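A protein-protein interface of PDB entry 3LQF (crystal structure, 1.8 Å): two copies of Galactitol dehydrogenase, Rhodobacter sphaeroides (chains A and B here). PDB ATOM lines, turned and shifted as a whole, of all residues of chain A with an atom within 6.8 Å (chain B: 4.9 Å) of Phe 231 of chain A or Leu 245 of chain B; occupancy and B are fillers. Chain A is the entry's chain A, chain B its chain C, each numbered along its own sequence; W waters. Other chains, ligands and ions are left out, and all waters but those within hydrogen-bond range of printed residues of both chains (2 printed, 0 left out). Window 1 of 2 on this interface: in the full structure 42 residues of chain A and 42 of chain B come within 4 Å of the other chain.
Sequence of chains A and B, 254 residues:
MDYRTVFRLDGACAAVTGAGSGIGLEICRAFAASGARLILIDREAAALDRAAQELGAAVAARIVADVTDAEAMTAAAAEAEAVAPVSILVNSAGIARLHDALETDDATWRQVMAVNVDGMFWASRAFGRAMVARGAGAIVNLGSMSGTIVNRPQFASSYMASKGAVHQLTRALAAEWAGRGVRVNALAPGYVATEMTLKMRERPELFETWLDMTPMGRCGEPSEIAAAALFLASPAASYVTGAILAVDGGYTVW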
ATOM      1  N   VAL A   6     -22.653  -0.653 -28.989  1.00  0.00           N
ATOM      2  CA  VAL A   6     -21.892   0.226 -28.089  1.00  0.00           C
ATOM      3  C   VAL A   6     -21.947  -0.190 -26.596  1.00  0.00           C
ATOM      4  O   VAL A   6     -21.040   0.147 -25.825  1.00  0.00           O
ATOM      5  CB  VAL A   6     -22.271   1.741 -28.286  1.00  0.00           C
ATOM      6  CG1 VAL A   6     -23.591   2.089 -27.556  1.00  0.00           C
ATOM      7  CG2 VAL A   6     -21.098   2.662 -27.876  1.00  0.00           C
ATOM      8  N   PHE A   7     -22.980  -0.935 -26.207  1.00  0.00           N
ATOM      9  CA  PHE A   7     -23.092  -1.413 -24.828  1.00  0.00           C
ATOM     10  C   PHE A   7     -22.421  -2.775 -24.590  1.00  0.00           C
ATOM     11  O   PHE A   7     -22.469  -3.288 -23.472  1.00  0.00           O
ATOM     12  CB  PHE A   7     -24.540  -1.482 -24.403  1.00  0.00           C
ATOM     13  CG  PHE A   7     -25.257  -0.165 -24.488  1.00  0.00           C
ATOM     14  CD1 PHE A   7     -25.156   0.768 -23.458  1.00  0.00           C
ATOM     15  CD2 PHE A   7     -26.055   0.118 -25.585  1.00  0.00           C
ATOM     16  CE1 PHE A   7     -25.833   1.984 -23.535  1.00  0.00           C
ATOM     17  CE2 PHE A   7     -26.725   1.320 -25.686  1.00  0.00           C
ATOM     18  CZ  PHE A   7     -26.624   2.260 -24.659  1.00  0.00           C
ATOM     19  N   PHE A  31     -22.165  -8.982 -17.384  1.00  0.00           N
ATOM     20  CA  PHE A  31     -20.937  -8.810 -18.181  1.00  0.00           C
ATOM     21  C   PHE A  31     -20.677 -10.022 -19.078  1.00  0.00           C
ATOM     22  O   PHE A  31     -20.224  -9.882 -20.231  1.00  0.00           O
ATOM     23  CB  PHE A  31     -19.749  -8.541 -17.252  1.00  0.00           C
ATOM     24  CG  PHE A  31     -19.706  -7.107 -16.698  1.00  0.00           C
ATOM     25  CD1 PHE A  31     -20.851  -6.284 -16.720  1.00  0.00           C
ATOM     26  CD2 PHE A  31     -18.537  -6.617 -16.123  1.00  0.00           C
ATOM     27  CE1 PHE A  31     -20.787  -4.977 -16.221  1.00  0.00           C
ATOM     28  CE2 PHE A  31     -18.459  -5.306 -15.622  1.00  0.00           C
ATOM     29  CZ  PHE A  31     -19.581  -4.494 -15.664  1.00  0.00           C
ATOM     30  N   VAL A 140     -15.684   0.515 -12.197  1.00  0.00           N
ATOM     31  CA  VAL A 140     -17.016   0.854 -11.698  1.00  0.00           C
ATOM     32  C   VAL A 140     -17.056   0.447 -10.232  1.00  0.00           C
ATOM     33  O   VAL A 140     -16.905  -0.731  -9.899  1.00  0.00           O
ATOM     34  CB  VAL A 140     -18.160   0.126 -12.431  1.00  0.00           C
ATOM     35  CG1 VAL A 140     -19.577   0.486 -11.783  1.00  0.00           C
ATOM     36  CG2 VAL A 140     -18.177   0.407 -13.948  1.00  0.00           C
ATOM     37  N   ARG A 183     -11.281   5.285 -17.211  1.00  0.00           N
ATOM     38  CA  ARG A 183     -12.457   5.982 -16.653  1.00  0.00           C
ATOM     39  C   ARG A 183     -12.782   5.338 -15.328  1.00  0.00           C
ATOM     40  O   ARG A 183     -12.584   4.127 -15.153  1.00  0.00           O
ATOM     41  CB  ARG A 183     -13.645   5.855 -17.596  1.00  0.00           C
ATOM     42  CG  ARG A 183     -13.410   6.480 -18.962  1.00  0.00           C
ATOM     43  CD  ARG A 183     -14.710   6.499 -19.780  1.00  0.00           C
ATOM     44  NE  ARG A 183     -15.100   5.134 -20.128  1.00  0.00           N
ATOM     45  CZ  ARG A 183     -16.052   4.442 -19.515  1.00  0.00           C
ATOM     46  NH1 ARG A 183     -16.766   4.995 -18.538  1.00  0.00           N
ATOM     47  NH2 ARG A 183     -16.300   3.196 -19.888  1.00  0.00           N
ATOM     48  N   ASN A 185     -15.872   5.507 -12.404  1.00  0.00           N
ATOM     49  CA  ASN A 185     -17.209   5.984 -12.005  1.00  0.00           C
ATOM     50  C   ASN A 185     -17.790   5.134 -10.887  1.00  0.00           C
ATOM     51  O   ASN A 185     -17.352   4.004 -10.661  1.00  0.00           O
ATOM     52  CB  ASN A 185     -18.176   5.946 -13.207  1.00  0.00           C
ATOM     53  CG  ASN A 185     -17.712   6.838 -14.345  1.00  0.00           C
ATOM     54  OD1 ASN A 185     -17.818   8.069 -14.266  1.00  0.00           O
ATOM     55  ND2 ASN A 185     -17.171   6.222 -15.419  1.00  0.00           N
ATOM     56  N   ALA A 226     -27.077  -3.885 -11.934  1.00  0.00           N
ATOM     57  CA  ALA A 226     -26.153  -4.450 -12.917  1.00  0.00           C
ATOM     58  C   ALA A 226     -26.262  -3.824 -14.284  1.00  0.00           C
ATOM     59  O   ALA A 226     -25.243  -3.655 -14.950  1.00  0.00           O
ATOM     60  CB  ALA A 226     -26.287  -5.975 -13.016  1.00  0.00           C
ATOM     61  N   ALA A 227     -27.473  -3.479 -14.725  1.00  0.00           N
ATOM     62  CA  ALA A 227     -27.601  -2.860 -16.050  1.00  0.00           C
ATOM     63  C   ALA A 227     -26.910  -1.481 -16.083  1.00  0.00           C
ATOM     64  O   ALA A 227     -26.289  -1.087 -17.086  1.00  0.00           O
ATOM     65  CB  ALA A 227     -29.042  -2.746 -16.459  1.00  0.00           C
ATOM     66  N   ALA A 228     -26.997  -0.768 -14.976  1.00  0.00           N
ATOM     67  CA  ALA A 228     -26.329   0.551 -14.884  1.00  0.00           C
ATOM     68  C   ALA A 228     -24.806   0.384 -14.836  1.00  0.00           C
ATOM     69  O   ALA A 228     -24.063   1.193 -15.407  1.00  0.00           O
ATOM     70  CB  ALA A 228     -26.817   1.309 -13.688  1.00  0.00           C
ATOM     71  N   ALA A 229     -24.350  -0.655 -14.137  1.00  0.00           N
ATOM     72  CA  ALA A 229     -22.919  -0.959 -14.056  1.00  0.00           C
ATOM     73  C   ALA A 229     -22.391  -1.285 -15.435  1.00  0.00           C
ATOM     74  O   ALA A 229     -21.274  -0.856 -15.820  1.00  0.00           O
ATOM     75  CB  ALA A 229     -22.674  -2.173 -13.090  1.00  0.00           C
ATOM     76  N   LEU A 230     -23.181  -2.078 -16.167  1.00  0.00           N
ATOM     77  CA  LEU A 230     -22.834  -2.414 -17.547  1.00  0.00           C
ATOM     78  C   LEU A 230     -22.659  -1.165 -18.410  1.00  0.00           C
ATOM     79  O   LEU A 230     -21.672  -1.043 -19.143  1.00  0.00           O
ATOM     80  CB  LEU A 230     -23.890  -3.352 -18.142  1.00  0.00           C
ATOM     81  CG  LEU A 230     -23.829  -3.744 -19.612  1.00  0.00           C
ATOM     82  CD1 LEU A 230     -22.481  -4.397 -19.914  1.00  0.00           C
ATOM     83  CD2 LEU A 230     -25.005  -4.711 -19.923  1.00  0.00           C
ATOM     84  N   PHE A 231     -23.608  -0.238 -18.317  1.00  0.00           N
ATOM     85  CA  PHE A 231     -23.511   1.043 -19.051  1.00  0.00           C
ATOM     86  C   PHE A 231     -22.174   1.720 -18.746  1.00  0.00           C
ATOM     87  O   PHE A 231     -21.416   2.069 -19.655  1.00  0.00           O
ATOM     88  CB  PHE A 231     -24.660   1.991 -18.673  1.00  0.00           C
ATOM     89  CG  PHE A 231     -24.397   3.424 -19.086  1.00  0.00           C
ATOM     90  CD1 PHE A 231     -24.219   3.743 -20.432  1.00  0.00           C
ATOM     91  CD2 PHE A 231     -24.273   4.441 -18.127  1.00  0.00           C
ATOM     92  CE1 PHE A 231     -23.934   5.045 -20.837  1.00  0.00           C
ATOM     93  CE2 PHE A 231     -24.001   5.747 -18.515  1.00  0.00           C
ATOM     94  CZ  PHE A 231     -23.832   6.058 -19.883  1.00  0.00           C
ATOM     95  N   LEU A 232     -21.885   1.890 -17.456  1.00  0.00           N
ATOM     96  CA  LEU A 232     -20.653   2.586 -17.043  1.00  0.00           C
ATOM     97  C   LEU A 232     -19.370   1.886 -17.506  1.00  0.00           C
ATOM     98  O   LEU A 232     -18.355   2.547 -17.760  1.00  0.00           O
ATOM     99  CB  LEU A 232     -20.627   2.781 -15.511  1.00  0.00           C
ATOM    100  CG  LEU A 232     -21.675   3.765 -14.972  1.00  0.00           C
ATOM    101  CD1 LEU A 232     -21.598   3.857 -13.454  1.00  0.00           C
ATOM    102  CD2 LEU A 232     -21.474   5.154 -15.588  1.00  0.00           C
ATOM    103  N   ALA A 233     -19.409   0.550 -17.596  1.00  0.00           N
ATOM    104  CA  ALA A 233     -18.211  -0.202 -17.944  1.00  0.00           C
ATOM    105  C   ALA A 233     -18.011  -0.212 -19.441  1.00  0.00           C
ATOM    106  O   ALA A 233     -16.926  -0.561 -19.903  1.00  0.00           O
ATOM    107  CB  ALA A 233     -18.302  -1.646 -17.429  1.00  0.00           C
ATOM    108  N   SER A 234     -19.068   0.106 -20.193  1.00  0.00           N
ATOM    109  CA  SER A 234     -19.040  -0.072 -21.648  1.00  0.00           C
ATOM    110  C   SER A 234     -18.544   1.178 -22.361  1.00  0.00           C
ATOM    111  O   SER A 234     -18.515   2.256 -21.781  1.00  0.00           O
ATOM    112  CB  SER A 234     -20.431  -0.441 -22.174  1.00  0.00           C
ATOM    113  OG  SER A 234     -21.309   0.679 -22.172  1.00  0.00           O
ATOM    114  N   PRO A 235     -18.196   1.039 -23.655  1.00  0.00           N
ATOM    115  CA  PRO A 235     -17.863   2.199 -24.492  1.00  0.00           C
ATOM    116  C   PRO A 235     -18.993   3.217 -24.661  1.00  0.00           C
ATOM    117  O   PRO A 235     -18.722   4.364 -25.044  1.00  0.00           O
ATOM    118  CB  PRO A 235     -17.514   1.557 -25.851  1.00  0.00           C
ATOM    119  CG  PRO A 235     -17.123   0.201 -25.530  1.00  0.00           C
ATOM    120  CD  PRO A 235     -17.968  -0.226 -24.375  1.00  0.00           C
ATOM    121  N   ALA A 236     -20.242   2.840 -24.362  1.00  0.00           N
ATOM    122  CA  ALA A 236     -21.327   3.826 -24.331  1.00  0.00           C
ATOM    123  C   ALA A 236     -21.019   4.995 -23.394  1.00  0.00           C
ATOM    124  O   ALA A 236     -21.467   6.126 -23.661  1.00  0.00           O
ATOM    125  CB  ALA A 236     -22.650   3.186 -23.944  1.00  0.00           C
ATOM    126  N   ALA A 237     -20.303   4.711 -22.292  1.00  0.00           N
ATOM    127  CA  ALA A 237     -19.987   5.713 -21.249  1.00  0.00           C
ATOM    128  C   ALA A 237     -18.608   6.358 -21.478  1.00  0.00           C
ATOM    129  O   ALA A 237     -17.965   6.801 -20.533  1.00  0.00           O
ATOM    130  CB  ALA A 237     -20.064   5.085 -19.820  1.00  0.00           C
ATOM    131  N   SER A 238     -18.178   6.443 -22.741  1.00  0.00           N
ATOM    132  CA  SER A 238     -16.788   6.844 -23.056  1.00  0.00           C
ATOM    133  C   SER A 238     -16.459   8.297 -22.667  1.00  0.00           C
ATOM    134  O   SER A 238     -15.289   8.643 -22.529  1.00  0.00           O
ATOM    135  CB  SER A 238     -16.463   6.632 -24.533  1.00  0.00           C
ATOM    136  OG  SER A 238     -17.388   7.311 -25.340  1.00  0.00           O
ATOM    137  N   VAL A 240     -17.903   9.579 -19.842  1.00  0.00           N
ATOM    138  CA  VAL A 240     -18.307   9.619 -18.421  1.00  0.00           C
ATOM    139  C   VAL A 240     -17.124   9.218 -17.565  1.00  0.00           C
ATOM    140  O   VAL A 240     -16.639   8.084 -17.644  1.00  0.00           O
ATOM    141  CB  VAL A 240     -19.499   8.726 -18.133  1.00  0.00           C
ATOM    142  CG1 VAL A 240     -20.055   8.986 -16.683  1.00  0.00           C
ATOM    143  CG2 VAL A 240     -20.624   8.942 -19.191  1.00  0.00           C
ATOM    144  N   ALA A 243     -18.158  10.340 -12.495  1.00  0.00           N
ATOM    145  CA  ALA A 243     -19.576  10.533 -12.156  1.00  0.00           C
ATOM    146  C   ALA A 243     -20.059   9.642 -11.022  1.00  0.00           C
ATOM    147  O   ALA A 243     -19.600   8.506 -10.836  1.00  0.00           O
ATOM    148  CB  ALA A 243     -20.472  10.349 -13.388  1.00  0.00           C
ATOM    149  N   ILE A 244     -21.013  10.163 -10.266  1.00  0.00           N
ATOM    150  CA  ILE A 244     -21.702   9.359  -9.284  1.00  0.00           C
ATOM    151  C   ILE A 244     -23.121   9.246  -9.817  1.00  0.00           C
ATOM    152  O   ILE A 244     -23.849  10.254  -9.869  1.00  0.00           O
ATOM    153  CB  ILE A 244     -21.711  10.062  -7.915  1.00  0.00           C
ATOM    154  CG1 ILE A 244     -20.299  10.505  -7.463  1.00  0.00           C
ATOM    155  CG2 ILE A 244     -22.504   9.210  -6.863  1.00  0.00           C
ATOM    156  CD1 ILE A 244     -19.203   9.365  -7.292  1.00  0.00           C
ATOM    157  N   LEU A 245     -23.510   8.047 -10.253  1.00  0.00           N
ATOM    158  CA  LEU A 245     -24.837   7.863 -10.863  1.00  0.00           C
ATOM    159  C   LEU A 245     -25.791   7.280  -9.847  1.00  0.00           C
ATOM    160  O   LEU A 245     -25.586   6.133  -9.422  1.00  0.00           O
ATOM    161  CB  LEU A 245     -24.740   6.935 -12.093  1.00  0.00           C
ATOM    162  CG  LEU A 245     -26.069   6.424 -12.714  1.00  0.00           C
ATOM    163  CD1 LEU A 245     -26.972   7.593 -13.123  1.00  0.00           C
ATOM    164  CD2 LEU A 245     -25.761   5.514 -13.930  1.00  0.00           C
ATOM    165  N   ALA A 246     -26.827   8.049  -9.473  1.00  0.00           N
ATOM    166  CA  ALA A 246     -27.860   7.557  -8.544  1.00  0.00           C
ATOM    167  C   ALA A 246     -28.743   6.540  -9.252  1.00  0.00           C
ATOM    168  O   ALA A 246     -29.260   6.822 -10.335  1.00  0.00           O
ATOM    169  CB  ALA A 246     -28.750   8.720  -8.023  1.00  0.00           C
ATOM    170  N   PHE B   7     -30.941  -2.376 -23.588  1.00  0.00           N
ATOM    171  CA  PHE B   7     -30.765  -0.979 -23.962  1.00  0.00           C
ATOM    172  C   PHE B   7     -31.543  -0.605 -25.228  1.00  0.00           C
ATOM    173  O   PHE B   7     -31.491   0.541 -25.657  1.00  0.00           O
ATOM    174  CB  PHE B   7     -29.289  -0.657 -24.175  1.00  0.00           C
ATOM    175  CG  PHE B   7     -28.407  -0.987 -22.997  1.00  0.00           C
ATOM    176  CD1 PHE B   7     -28.319  -0.126 -21.900  1.00  0.00           C
ATOM    177  CD2 PHE B   7     -27.635  -2.138 -23.001  1.00  0.00           C
ATOM    178  CE1 PHE B   7     -27.488  -0.413 -20.817  1.00  0.00           C
ATOM    179  CE2 PHE B   7     -26.794  -2.432 -21.938  1.00  0.00           C
ATOM    180  CZ  PHE B   7     -26.729  -1.567 -20.832  1.00  0.00           C
ATOM    181  N   ALA B 186     -31.948  13.613 -16.095  1.00  0.00           N
ATOM    182  CA  ALA B 186     -31.221  14.591 -16.927  1.00  0.00           C
ATOM    183  C   ALA B 186     -29.801  14.186 -17.217  1.00  0.00           C
ATOM    184  O   ALA B 186     -29.113  13.608 -16.357  1.00  0.00           O
ATOM    185  CB  ALA B 186     -31.227  15.995 -16.279  1.00  0.00           C
ATOM    186  N   LEU B 187     -29.344  14.500 -18.428  1.00  0.00           N
ATOM    187  CA  LEU B 187     -27.933  14.518 -18.703  1.00  0.00           C
ATOM    188  C   LEU B 187     -27.329  15.885 -18.355  1.00  0.00           C
ATOM    189  O   LEU B 187     -27.927  16.932 -18.635  1.00  0.00           O
ATOM    190  CB  LEU B 187     -27.657  14.222 -20.195  1.00  0.00           C
ATOM    191  CG  LEU B 187     -28.113  12.817 -20.630  1.00  0.00           C
ATOM    192  CD1 LEU B 187     -28.082  12.705 -22.147  1.00  0.00           C
ATOM    193  CD2 LEU B 187     -27.264  11.724 -19.958  1.00  0.00           C
ATOM    194  N   ALA B 188     -26.126  15.876 -17.800  1.00  0.00           N
ATOM    195  CA  ALA B 188     -25.383  17.129 -17.600  1.00  0.00           C
ATOM    196  C   ALA B 188     -24.104  17.085 -18.424  1.00  0.00           C
ATOM    197  O   ALA B 188     -23.050  16.731 -17.888  1.00  0.00           O
ATOM    198  CB  ALA B 188     -25.047  17.341 -16.094  1.00  0.00           C
ATOM    199  N   ALA B 227     -25.492   8.244 -26.543  1.00  0.00           N
ATOM    200  CA  ALA B 227     -25.421   6.895 -25.952  1.00  0.00           C
ATOM    201  C   ALA B 227     -25.908   6.933 -24.505  1.00  0.00           C
ATOM    202  O   ALA B 227     -26.581   6.031 -24.049  1.00  0.00           O
ATOM    203  CB  ALA B 227     -24.012   6.334 -26.032  1.00  0.00           C
ATOM    204  N   ALA B 228     -25.571   8.012 -23.797  1.00  0.00           N
ATOM    205  CA  ALA B 228     -26.027   8.179 -22.420  1.00  0.00           C
ATOM    206  C   ALA B 228     -27.528   8.440 -22.344  1.00  0.00           C
ATOM    207  O   ALA B 228     -28.204   7.896 -21.461  1.00  0.00           O
ATOM    208  CB  ALA B 228     -25.197   9.302 -21.698  1.00  0.00           C
ATOM    209  N   PHE B 231     -29.204   5.059 -22.801  1.00  0.00           N
ATOM    210  CA  PHE B 231     -29.248   4.420 -21.490  1.00  0.00           C
ATOM    211  C   PHE B 231     -30.452   4.901 -20.660  1.00  0.00           C
ATOM    212  O   PHE B 231     -31.275   4.095 -20.245  1.00  0.00           O
ATOM    213  CB  PHE B 231     -27.933   4.634 -20.702  1.00  0.00           C
ATOM    214  CG  PHE B 231     -28.034   4.191 -19.244  1.00  0.00           C
ATOM    215  CD1 PHE B 231     -28.328   2.869 -18.927  1.00  0.00           C
ATOM    216  CD2 PHE B 231     -27.854   5.104 -18.202  1.00  0.00           C
ATOM    217  CE1 PHE B 231     -28.471   2.445 -17.597  1.00  0.00           C
ATOM    218  CE2 PHE B 231     -27.976   4.696 -16.853  1.00  0.00           C
ATOM    219  CZ  PHE B 231     -28.273   3.359 -16.549  1.00  0.00           C
ATOM    220  N   LEU B 232     -30.541   6.208 -20.392  1.00  0.00           N
ATOM    221  CA  LEU B 232     -31.617   6.744 -19.504  1.00  0.00           C
ATOM    222  C   LEU B 232     -33.031   6.548 -20.057  1.00  0.00           C
ATOM    223  O   LEU B 232     -33.984   6.424 -19.297  1.00  0.00           O
ATOM    224  CB  LEU B 232     -31.389   8.250 -19.235  1.00  0.00           C
ATOM    225  CG  LEU B 232     -30.116   8.609 -18.459  1.00  0.00           C
ATOM    226  CD1 LEU B 232     -29.930  10.141 -18.498  1.00  0.00           C
ATOM    227  CD2 LEU B 232     -30.151   8.025 -17.042  1.00  0.00           C
ATOM    228  N   ALA B 243     -32.238  11.380 -11.486  1.00  0.00           N
ATOM    229  CA  ALA B 243     -30.770  11.424 -11.526  1.00  0.00           C
ATOM    230  C   ALA B 243     -30.289  12.519 -12.451  1.00  0.00           C
ATOM    231  O   ALA B 243     -30.908  12.780 -13.481  1.00  0.00           O
ATOM    232  CB  ALA B 243     -30.200  10.067 -11.969  1.00  0.00           C
ATOM    233  N   ILE B 244     -29.185  13.162 -12.068  1.00  0.00           N
ATOM    234  CA  ILE B 244     -28.500  14.076 -12.926  1.00  0.00           C
ATOM    235  C   ILE B 244     -27.202  13.340 -13.269  1.00  0.00           C
ATOM    236  O   ILE B 244     -26.324  13.133 -12.386  1.00  0.00           O
ATOM    237  CB  ILE B 244     -28.181  15.454 -12.218  1.00  0.00           C
ATOM    238  CG1 ILE B 244     -29.423  16.108 -11.580  1.00  0.00           C
ATOM    239  CG2 ILE B 244     -27.443  16.365 -13.215  1.00  0.00           C
ATOM    240  CD1 ILE B 244     -30.671  16.270 -12.545  1.00  0.00           C
ATOM    241  N   LEU B 245     -27.083  12.921 -14.515  1.00  0.00           N
ATOM    242  CA  LEU B 245     -25.914  12.152 -14.962  1.00  0.00           C
ATOM    243  C   LEU B 245     -24.851  13.019 -15.658  1.00  0.00           C
ATOM    244  O   LEU B 245     -25.100  13.506 -16.770  1.00  0.00           O
ATOM    245  CB  LEU B 245     -26.353  11.008 -15.896  1.00  0.00           C
ATOM    246  CG  LEU B 245     -25.192  10.224 -16.562  1.00  0.00           C
ATOM    247  CD1 LEU B 245     -24.257   9.623 -15.519  1.00  0.00           C
ATOM    248  CD2 LEU B 245     -25.806   9.140 -17.443  1.00  0.00           C
ATOM    249  N   ALA B 246     -23.690  13.199 -15.000  1.00  0.00           N
ATOM    250  CA  ALA B 246     -22.581  13.967 -15.569  1.00  0.00           C
ATOM    251  C   ALA B 246     -22.011  13.178 -16.714  1.00  0.00           C
ATOM    252  O   ALA B 246     -21.718  11.988 -16.570  1.00  0.00           O
ATOM    253  CB  ALA B 246     -21.470  14.269 -14.510  1.00  0.00           C
ATOM    254  N   VAL B 247     -21.914  13.829 -17.872  1.00  0.00           N
ATOM    255  CA  VAL B 247     -21.273  13.213 -19.037  1.00  0.00           C
ATOM    256  C   VAL B 247     -20.360  14.318 -19.538  1.00  0.00           C
ATOM    257  O   VAL B 247     -20.668  14.981 -20.525  1.00  0.00           O
ATOM    258  CB  VAL B 247     -22.286  12.796 -20.155  1.00  0.00           C
ATOM    259  CG1 VAL B 247     -21.513  12.138 -21.333  1.00  0.00           C
ATOM    260  CG2 VAL B 247     -23.340  11.840 -19.627  1.00  0.00           C
HETATM  261  O   HOH W   1     -23.532  12.161 -12.275  1.00  0.00           O
HETATM  262  O   HOH W   2     -26.788  10.776 -10.280  1.00  0.00           O
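The backbone carbonyl oxygen (O) of Val 240 of chain A lies within hydrogen-bond range of the guanidinium group (NH1) of Arg 183 of chain A (3.2 Å).
N of Ala 243 of chain A is in hydrogen-bond range of OD1 of Asn 185 of chain A, at 2.9 Å.
The backbone carbonyl oxygen (O) of Phe 231 of chain A is in hydrogen-bond range of the side-chain hydroxyl (OG) of Ser 234 of chain A.
The backbone NH (N) of Ala 186 of chain B lies within hydrogen-bond range of the backbone carbonyl oxygen (O) of Ala 243 of chain B (2.9 Å).
O of Leu 245 of chain B sits at hydrogen-bond distance from N of Ala 188 of chain B, 2.8 Å away.
N of Val 247 of chain B sits at hydrogen-bond distance from O of Ala 188 of chain B (3.1 Å).
Phe 7 of chain B touches Phe 7 of chain A (CD2 to CG, 3.4 Å).
O of Ala 227 of chain B touches CZ of Phe 7 of chain A (3.8 Å).
Phe 7 of chain B touches Ala 227 of chain A (CZ to O, 3.8 Å).
Ala 228 of chain A touches Phe 231 of chain B (CA to CZ, 3.8 Å).
Phe 7 of chain B touches Leu 230 of chain A.
Ala 228 of chain B touches Phe 231 of chain A.
O of Ala 246 of chain B touches CG1 of Val 240 of chain A, at 3.4 Å.
Val 240 of chain A touches Val 247 of chain B.
CB of Ala 243 of chain A touches O of Ala 246 of chain B, 3.8 Å away.
Phe 231 of chain B touches Leu 245 of chain A (CE2 to CD2, 3.8 Å).
Printed residues of chain B within 4 Å of Leu 230 of chain A: Phe 7 (3.5 Å).
Of the printed residues of chain B, Phe 231 of chain A touches Ala 228, Phe 231 and Leu 245.
Printed residues of chain B within 4 Å of Val 240 of chain A: Ala 246 and Val 247.
Printed residues of chain B within 4 Å of Ala 243 of chain A: Ala 246.
Ile 244 of chain A touches none of the printed residues of chain B.
Of the printed residues of chain B, Ala 246 of chain A touches Ala 243 (3.8 Å).
Of the printed residues of chain A, Ala 246 of chain B touches Val 240 and Ala 243.
The nearest printed residue of chain B that does not touch Phe 231 of chain A is Phe 7 of chain B (4.2 Å).
The nearest printed residue of chain A that does not touch Leu 245 of chain B is Leu 245 of chain A (4.2 Å).
Of the 13 printed residues of chain B, 8 touch a printed residue of chain A.
Hydrophobic or aromatic side chains of chain B within 4 Å of the printed part of chain A: Phe 7, Ala 227, Ala 228, Phe 231, Ala 243, Leu 245 and Val 247.
Hydrophobic or aromatic side chains of chain A that line the printed part of chain B: Phe 7, Ala 228, Leu 230, Phe 231, Val 240, Ala 243 and Leu 245.
Among the printed residues, no Asp or Glu carboxylate lies within 4 Å of a Lys or Arg side-chain nitrogen of the other chain.
Phe 7 of chain B touches its own counterpart, Phe 7 of chain A.
Ala 228 of chain A touches Phe 231 of chain B, and with the chains exchanged Phe 231 of chain A touches Ala 228 of chain B.
Phe 231 of chain B touches its own counterpart, Phe 231 of chain A.
Phe 231 of chain A touches Leu 245 of chain B, and with the chains exchanged Leu 245 of chain A touches Phe 231 of chain B.
Water W2 lies within hydrogen-bond range of N of Ala 246 of chain A, O of Ile 244 of chain A and O of Ile 244 of chain B.
Water W1 lies within hydrogen-bond range of N of Ala 246 of chain B (2.9 Å), O of Ile 244 of chain B (3.0 Å) and O of Ile 244 of chain A (3.1 Å).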
